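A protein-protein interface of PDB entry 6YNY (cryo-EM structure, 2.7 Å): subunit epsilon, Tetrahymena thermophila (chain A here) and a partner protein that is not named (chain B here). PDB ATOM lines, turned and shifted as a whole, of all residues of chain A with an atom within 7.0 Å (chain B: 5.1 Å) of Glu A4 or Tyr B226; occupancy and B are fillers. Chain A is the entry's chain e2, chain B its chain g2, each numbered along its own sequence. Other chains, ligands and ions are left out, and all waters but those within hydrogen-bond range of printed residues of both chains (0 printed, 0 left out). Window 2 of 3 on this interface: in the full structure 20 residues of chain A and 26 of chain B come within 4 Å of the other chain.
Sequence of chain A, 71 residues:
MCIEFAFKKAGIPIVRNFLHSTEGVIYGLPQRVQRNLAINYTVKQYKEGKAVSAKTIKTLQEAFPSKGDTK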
ATOM      1  N   CYS A   2      16.111  24.338 -19.193  1.00  0.00           N
ATOM      2  CA  CYS A   2      15.791  23.644 -17.951  1.00  0.00           C
ATOM      3  C   CYS A   2      17.063  23.253 -17.211  1.00  0.00           C
ATOM      4  O   CYS A   2      17.943  22.602 -17.770  1.00  0.00           O
ATOM      5  CB  CYS A   2      14.942  22.402 -18.232  1.00  0.00           C
ATOM      6  SG  CYS A   2      15.703  21.218 -19.366  1.00  0.00           S
ATOM      7  N   ILE A   3      17.153  23.659 -15.944  1.00  0.00           N
ATOM      8  CA  ILE A   3      18.336  23.339 -15.154  1.00  0.00           C
ATOM      9  C   ILE A   3      18.214  21.956 -14.531  1.00  0.00           C
ATOM     10  O   ILE A   3      19.228  21.300 -14.264  1.00  0.00           O
ATOM     11  CB  ILE A   3      18.566  24.416 -14.081  1.00  0.00           C
ATOM     12  CG1 ILE A   3      17.483  24.348 -13.004  1.00  0.00           C
ATOM     13  CG2 ILE A   3      18.567  25.791 -14.714  1.00  0.00           C
ATOM     14  CD1 ILE A   3      17.610  25.424 -11.950  1.00  0.00           C
ATOM     15  N   GLU A   4      16.990  21.490 -14.285  1.00  0.00           N
ATOM     16  CA  GLU A   4      16.800  20.213 -13.609  1.00  0.00           C
ATOM     17  C   GLU A   4      17.046  19.043 -14.555  1.00  0.00           C
ATOM     18  O   GLU A   4      17.861  18.161 -14.263  1.00  0.00           O
ATOM     19  CB  GLU A   4      15.394  20.145 -13.007  1.00  0.00           C
ATOM     20  CG  GLU A   4      14.260  20.312 -14.005  1.00  0.00           C
ATOM     21  CD  GLU A   4      12.914  20.488 -13.331  1.00  0.00           C
ATOM     22  OE1 GLU A   4      12.863  20.442 -12.084  1.00  0.00           O
ATOM     23  OE2 GLU A   4      11.908  20.675 -14.046  1.00  0.00           O
ATOM     24  N   PHE A   5      16.361  19.022 -15.701  1.00  0.00           N
ATOM     25  CA  PHE A   5      16.529  17.911 -16.630  1.00  0.00           C
ATOM     26  C   PHE A   5      17.897  17.939 -17.295  1.00  0.00           C
ATOM     27  O   PHE A   5      18.414  16.885 -17.683  1.00  0.00           O
ATOM     28  CB  PHE A   5      15.426  17.935 -17.689  1.00  0.00           C
ATOM     29  CG  PHE A   5      14.111  17.383 -17.214  1.00  0.00           C
ATOM     30  CD1 PHE A   5      14.048  16.162 -16.564  1.00  0.00           C
ATOM     31  CD2 PHE A   5      12.937  18.086 -17.420  1.00  0.00           C
ATOM     32  CE1 PHE A   5      12.844  15.654 -16.129  1.00  0.00           C
ATOM     33  CE2 PHE A   5      11.728  17.583 -16.986  1.00  0.00           C
ATOM     34  CZ  PHE A   5      11.681  16.365 -16.341  1.00  0.00           C
ATOM     35  N   ALA A   6      18.496  19.123 -17.436  1.00  0.00           N
ATOM     36  CA  ALA A   6      19.835  19.193 -18.007  1.00  0.00           C
ATOM     37  C   ALA A   6      20.826  18.379 -17.191  1.00  0.00           C
ATOM     38  O   ALA A   6      21.832  17.904 -17.729  1.00  0.00           O
ATOM     39  CB  ALA A   6      20.292  20.648 -18.100  1.00  0.00           C
ATOM     40  N   PHE A   7      20.565  18.209 -15.895  1.00  0.00           N
ATOM     41  CA  PHE A   7      21.437  17.414 -15.043  1.00  0.00           C
ATOM     42  C   PHE A   7      20.977  15.971 -14.927  1.00  0.00           C
ATOM     43  O   PHE A   7      21.806  15.079 -14.713  1.00  0.00           O
ATOM     44  CB  PHE A   7      21.514  18.034 -13.647  1.00  0.00           C
ATOM     45  CG  PHE A   7      22.297  17.215 -12.663  1.00  0.00           C
ATOM     46  CD1 PHE A   7      23.679  17.271 -12.640  1.00  0.00           C
ATOM     47  CD2 PHE A   7      21.651  16.397 -11.754  1.00  0.00           C
ATOM     48  CE1 PHE A   7      24.401  16.521 -11.733  1.00  0.00           C
ATOM     49  CE2 PHE A   7      22.368  15.647 -10.845  1.00  0.00           C
ATOM     50  CZ  PHE A   7      23.743  15.709 -10.834  1.00  0.00           C
ATOM     51  N   LYS A   8      19.674  15.719 -15.059  1.00  0.00           N
ATOM     52  CA  LYS A   8      19.156  14.368 -14.883  1.00  0.00           C
ATOM     53  C   LYS A   8      19.426  13.513 -16.114  1.00  0.00           C
ATOM     54  O   LYS A   8      20.090  12.474 -16.034  1.00  0.00           O
ATOM     55  CB  LYS A   8      17.656  14.419 -14.582  1.00  0.00           C
ATOM     56  CG  LYS A   8      17.019  13.064 -14.306  1.00  0.00           C
ATOM     57  CD  LYS A   8      17.754  12.290 -13.214  1.00  0.00           C
ATOM     58  CE  LYS A   8      17.915  13.104 -11.936  1.00  0.00           C
ATOM     59  NZ  LYS A   8      18.573  12.319 -10.860  1.00  0.00           N
ATOM     60  N   LYS A   9      18.917  13.942 -17.268  1.00  0.00           N
ATOM     61  CA  LYS A   9      19.109  13.205 -18.509  1.00  0.00           C
ATOM     62  C   LYS A   9      20.477  13.449 -19.125  1.00  0.00           C
ATOM     63  O   LYS A   9      20.815  12.803 -20.123  1.00  0.00           O
ATOM     64  CB  LYS A   9      18.016  13.580 -19.511  1.00  0.00           C
ATOM     65  CG  LYS A   9      17.802  12.555 -20.609  1.00  0.00           C
ATOM     66  CD  LYS A   9      16.555  12.867 -21.422  1.00  0.00           C
ATOM     67  CE  LYS A   9      16.254  11.769 -22.428  1.00  0.00           C
ATOM     68  NZ  LYS A   9      15.959  10.465 -21.770  1.00  0.00           N
ATOM     69  N   ALA A  10      21.267  14.356 -18.557  1.00  0.00           N
ATOM     70  CA  ALA A  10      22.609  14.638 -19.040  1.00  0.00           C
ATOM     71  C   ALA A  10      23.466  15.051 -17.854  1.00  0.00           C
ATOM     72  O   ALA A  10      22.991  15.743 -16.951  1.00  0.00           O
ATOM     73  CB  ALA A  10      22.601  15.739 -20.106  1.00  0.00           C
ATOM     74  N   ILE A  12      25.259  17.326 -16.881  1.00  0.00           N
ATOM     75  CA  ILE A  12      25.626  18.734 -16.991  1.00  0.00           C
ATOM     76  C   ILE A  12      25.584  19.336 -15.588  1.00  0.00           C
ATOM     77  O   ILE A  12      24.487  19.481 -15.023  1.00  0.00           O
ATOM     78  CB  ILE A  12      24.683  19.487 -17.938  1.00  0.00           C
ATOM     79  CG1 ILE A  12      24.608  18.774 -19.289  1.00  0.00           C
ATOM     80  CG2 ILE A  12      25.154  20.920 -18.122  1.00  0.00           C
ATOM     81  CD1 ILE A  12      23.624  19.395 -20.253  1.00  0.00           C
ATOM     82  N   ASN A  17      26.255  24.787 -16.757  1.00  0.00           N
ATOM     83  CA  ASN A  17      25.020  25.315 -17.326  1.00  0.00           C
ATOM     84  C   ASN A  17      25.046  26.838 -17.358  1.00  0.00           C
ATOM     85  O   ASN A  17      24.705  27.457 -18.373  1.00  0.00           O
ATOM     86  CB  ASN A  17      23.821  24.815 -16.524  1.00  0.00           C
ATOM     87  CG  ASN A  17      22.501  25.140 -17.190  1.00  0.00           C
ATOM     88  OD1 ASN A  17      22.461  25.555 -18.347  1.00  0.00           O
ATOM     89  ND2 ASN A  17      21.410  24.948 -16.460  1.00  0.00           N
ATOM     90  N   GLU B 221      11.577  24.134  -4.998  1.00  0.00           N
ATOM     91  CA  GLU B 221      11.745  24.828  -6.275  1.00  0.00           C
ATOM     92  C   GLU B 221      12.595  24.004  -7.230  1.00  0.00           C
ATOM     93  O   GLU B 221      12.093  23.612  -8.298  1.00  0.00           O
ATOM     94  CB  GLU B 221      12.311  26.228  -6.027  1.00  0.00           C
ATOM     95  CG  GLU B 221      11.310  27.202  -5.424  1.00  0.00           C
ATOM     96  CD  GLU B 221      10.130  27.475  -6.336  1.00  0.00           C
ATOM     97  OE1 GLU B 221      10.234  27.185  -7.546  1.00  0.00           O
ATOM     98  OE2 GLU B 221       9.099  27.980  -5.843  1.00  0.00           O
ATOM     99  N   PRO B 222      13.860  23.708  -6.932  1.00  0.00           N
ATOM    100  CA  PRO B 222      14.489  22.524  -7.520  1.00  0.00           C
ATOM    101  C   PRO B 222      14.321  21.341  -6.582  1.00  0.00           C
ATOM    102  O   PRO B 222      14.479  21.455  -5.365  1.00  0.00           O
ATOM    103  CB  PRO B 222      15.957  22.948  -7.645  1.00  0.00           C
ATOM    104  CG  PRO B 222      16.160  23.823  -6.473  1.00  0.00           C
ATOM    105  CD  PRO B 222      14.853  24.551  -6.243  1.00  0.00           C
ATOM    106  N   GLU B 223      13.993  20.189  -7.154  1.00  0.00           N
ATOM    107  CA  GLU B 223      13.744  19.031  -6.315  1.00  0.00           C
ATOM    108  C   GLU B 223      15.038  18.560  -5.660  1.00  0.00           C
ATOM    109  O   GLU B 223      16.145  18.845  -6.123  1.00  0.00           O
ATOM    110  CB  GLU B 223      13.111  17.903  -7.127  1.00  0.00           C
ATOM    111  CG  GLU B 223      11.694  18.199  -7.572  1.00  0.00           C
ATOM    112  CD  GLU B 223      10.719  18.250  -6.413  1.00  0.00           C
ATOM    113  OE1 GLU B 223      11.098  17.831  -5.298  1.00  0.00           O
ATOM    114  OE2 GLU B 223       9.577  18.711  -6.614  1.00  0.00           O
ATOM    115  N   LEU B 224      14.880  17.827  -4.557  1.00  0.00           N
ATOM    116  CA  LEU B 224      16.034  17.444  -3.752  1.00  0.00           C
ATOM    117  C   LEU B 224      17.055  16.669  -4.575  1.00  0.00           C
ATOM    118  O   LEU B 224      18.265  16.822  -4.377  1.00  0.00           O
ATOM    119  CB  LEU B 224      15.578  16.620  -2.551  1.00  0.00           C
ATOM    120  CG  LEU B 224      16.659  16.269  -1.530  1.00  0.00           C
ATOM    121  CD1 LEU B 224      17.278  17.528  -0.957  1.00  0.00           C
ATOM    122  CD2 LEU B 224      16.082  15.413  -0.421  1.00  0.00           C
ATOM    123  N   GLU B 225      16.589  15.832  -5.504  1.00  0.00           N
ATOM    124  CA  GLU B 225      17.519  15.047  -6.309  1.00  0.00           C
ATOM    125  C   GLU B 225      18.460  15.941  -7.104  1.00  0.00           C
ATOM    126  O   GLU B 225      19.612  15.564  -7.350  1.00  0.00           O
ATOM    127  CB  GLU B 225      16.750  14.119  -7.249  1.00  0.00           C
ATOM    128  CG  GLU B 225      15.895  14.838  -8.275  1.00  0.00           C
ATOM    129  CD  GLU B 225      15.075  13.882  -9.118  1.00  0.00           C
ATOM    130  OE1 GLU B 225      15.332  12.661  -9.056  1.00  0.00           O
ATOM    131  OE2 GLU B 225      14.171  14.350  -9.841  1.00  0.00           O
ATOM    132  N   TYR B 226      17.996  17.120  -7.514  1.00  0.00           N
ATOM    133  CA  TYR B 226      18.847  18.068  -8.220  1.00  0.00           C
ATOM    134  C   TYR B 226      19.605  18.975  -7.262  1.00  0.00           C
ATOM    135  O   TYR B 226      20.782  19.273  -7.488  1.00  0.00           O
ATOM    136  CB  TYR B 226      18.009  18.924  -9.171  1.00  0.00           C
ATOM    137  CG  TYR B 226      17.041  18.141 -10.022  1.00  0.00           C
ATOM    138  CD1 TYR B 226      17.420  17.629 -11.253  1.00  0.00           C
ATOM    139  CD2 TYR B 226      15.743  17.916  -9.594  1.00  0.00           C
ATOM    140  CE1 TYR B 226      16.534  16.914 -12.030  1.00  0.00           C
ATOM    141  CE2 TYR B 226      14.849  17.203 -10.365  1.00  0.00           C
ATOM    142  CZ  TYR B 226      15.250  16.703 -11.583  1.00  0.00           C
ATOM    143  OH  TYR B 226      14.363  15.991 -12.357  1.00  0.00           O
ATOM    144  N   SER B 227      18.945  19.421  -6.192  1.00  0.00           N
ATOM    145  CA  SER B 227      19.576  20.355  -5.268  1.00  0.00           C
ATOM    146  C   SER B 227      20.758  19.715  -4.554  1.00  0.00           C
ATOM    147  O   SER B 227      21.770  20.378  -4.300  1.00  0.00           O
ATOM    148  CB  SER B 227      18.549  20.855  -4.256  1.00  0.00           C
ATOM    149  OG  SER B 227      19.122  21.807  -3.379  1.00  0.00           O
ATOM    150  N   LYS B 228      20.649  18.428  -4.220  1.00  0.00           N
ATOM    151  CA  LYS B 228      21.724  17.764  -3.492  1.00  0.00           C
ATOM    152  C   LYS B 228      23.020  17.783  -4.290  1.00  0.00           C
ATOM    153  O   LYS B 228      24.098  18.014  -3.731  1.00  0.00           O
ATOM    154  CB  LYS B 228      21.314  16.330  -3.160  1.00  0.00           C
ATOM    155  CG  LYS B 228      21.097  15.451  -4.380  1.00  0.00           C
ATOM    156  CD  LYS B 228      20.263  14.225  -4.048  1.00  0.00           C
ATOM    157  CE  LYS B 228      20.941  13.331  -3.029  1.00  0.00           C
ATOM    158  NZ  LYS B 228      20.110  12.141  -2.703  1.00  0.00           N
ATOM    159  N   ASN B 229      22.936  17.545  -5.599  1.00  0.00           N
ATOM    160  CA  ASN B 229      24.136  17.526  -6.423  1.00  0.00           C
ATOM    161  C   ASN B 229      24.640  18.932  -6.719  1.00  0.00           C
ATOM    162  O   ASN B 229      25.852  19.137  -6.848  1.00  0.00           O
ATOM    163  CB  ASN B 229      23.863  16.781  -7.729  1.00  0.00           C
ATOM    164  CG  ASN B 229      23.402  15.356  -7.497  1.00  0.00           C
ATOM    165  OD1 ASN B 229      22.205  15.070  -7.509  1.00  0.00           O
ATOM    166  ND2 ASN B 229      24.352  14.455  -7.278  1.00  0.00           N
ATOM    167  N   TYR B 230      23.735  19.904  -6.829  1.00  0.00           N
ATOM    168  CA  TYR B 230      24.144  21.271  -7.129  1.00  0.00           C
ATOM    169  C   TYR B 230      24.891  21.885  -5.951  1.00  0.00           C
ATOM    170  O   TYR B 230      26.026  22.354  -6.093  1.00  0.00           O
ATOM    171  CB  TYR B 230      22.923  22.116  -7.493  1.00  0.00           C
ATOM    172  CG  TYR B 230      22.279  21.764  -8.817  1.00  0.00           C
ATOM    173  CD1 TYR B 230      22.821  20.793  -9.647  1.00  0.00           C
ATOM    174  CD2 TYR B 230      21.132  22.417  -9.242  1.00  0.00           C
ATOM    175  CE1 TYR B 230      22.234  20.478 -10.856  1.00  0.00           C
ATOM    176  CE2 TYR B 230      20.540  22.110 -10.449  1.00  0.00           C
ATOM    177  CZ  TYR B 230      21.094  21.141 -11.251  1.00  0.00           C
ATOM    178  OH  TYR B 230      20.502  20.836 -12.454  1.00  0.00           O
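The backbone carbonyl oxygen of Ile A3 sits close to the side-chain hydroxyl of Tyr B230, 2.3 Å away.
The side-chain amino group (NZ) of Lys A8 is in salt-bridge range of the side-chain carboxylate (OE1) of Glu B225 (3.7 Å).
The side-chain carboxylate of Glu B225 sits close to the side-chain hydroxyl of Tyr B226 (3.0 Å).
The side-chain amide oxygen (OD1) of Asn B229 lies close to the backbone carbonyl oxygen (O) of Glu B225, 2.6 Å away.
Glu A4 touches Tyr B226 (O to CE1, 2.9 Å).
Glu A4 touches Tyr B230.
Phe A7 touches Asn B229.
Phe A7 touches Tyr B230.
Lys A8 touches Tyr B226 (CB to CE1, 3.7 Å).
Printed residues of chain B within 4 Å of Glu A4: Tyr B226 (2.9 Å) and Tyr B230 (3.9 Å).
Of chain A, only Glu A4 (2.9 Å) and Lys A8 (3.7 Å) come within 4 Å of Tyr B226.
Printed residues of chain B within 4 Å of Ile A3: Tyr B230 (2.3 Å).
Printed residues of chain B within 4 Å of Lys A8: Glu B225 and Tyr B226.
Printed residues of chain A within 4 Å of Glu B225: Lys A8 (3.7 Å).
Printed residues of chain A within 4 Å of Tyr B230: Ile A3, Glu A4 and Phe A7.
The nearest residue of chain B that does not touch Glu A4 is Glu B221 (5.0 Å).
Of the 11 printed residues of chain A, 4 touch a printed residue of chain B.
Printed residues of chain A that touch a printed residue of chain B: Ile A3, Glu A4, Phe A7 and Lys A8.
Hydrophobic or aromatic side chains of chain A that line the printed part of chain B: Phe A7.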
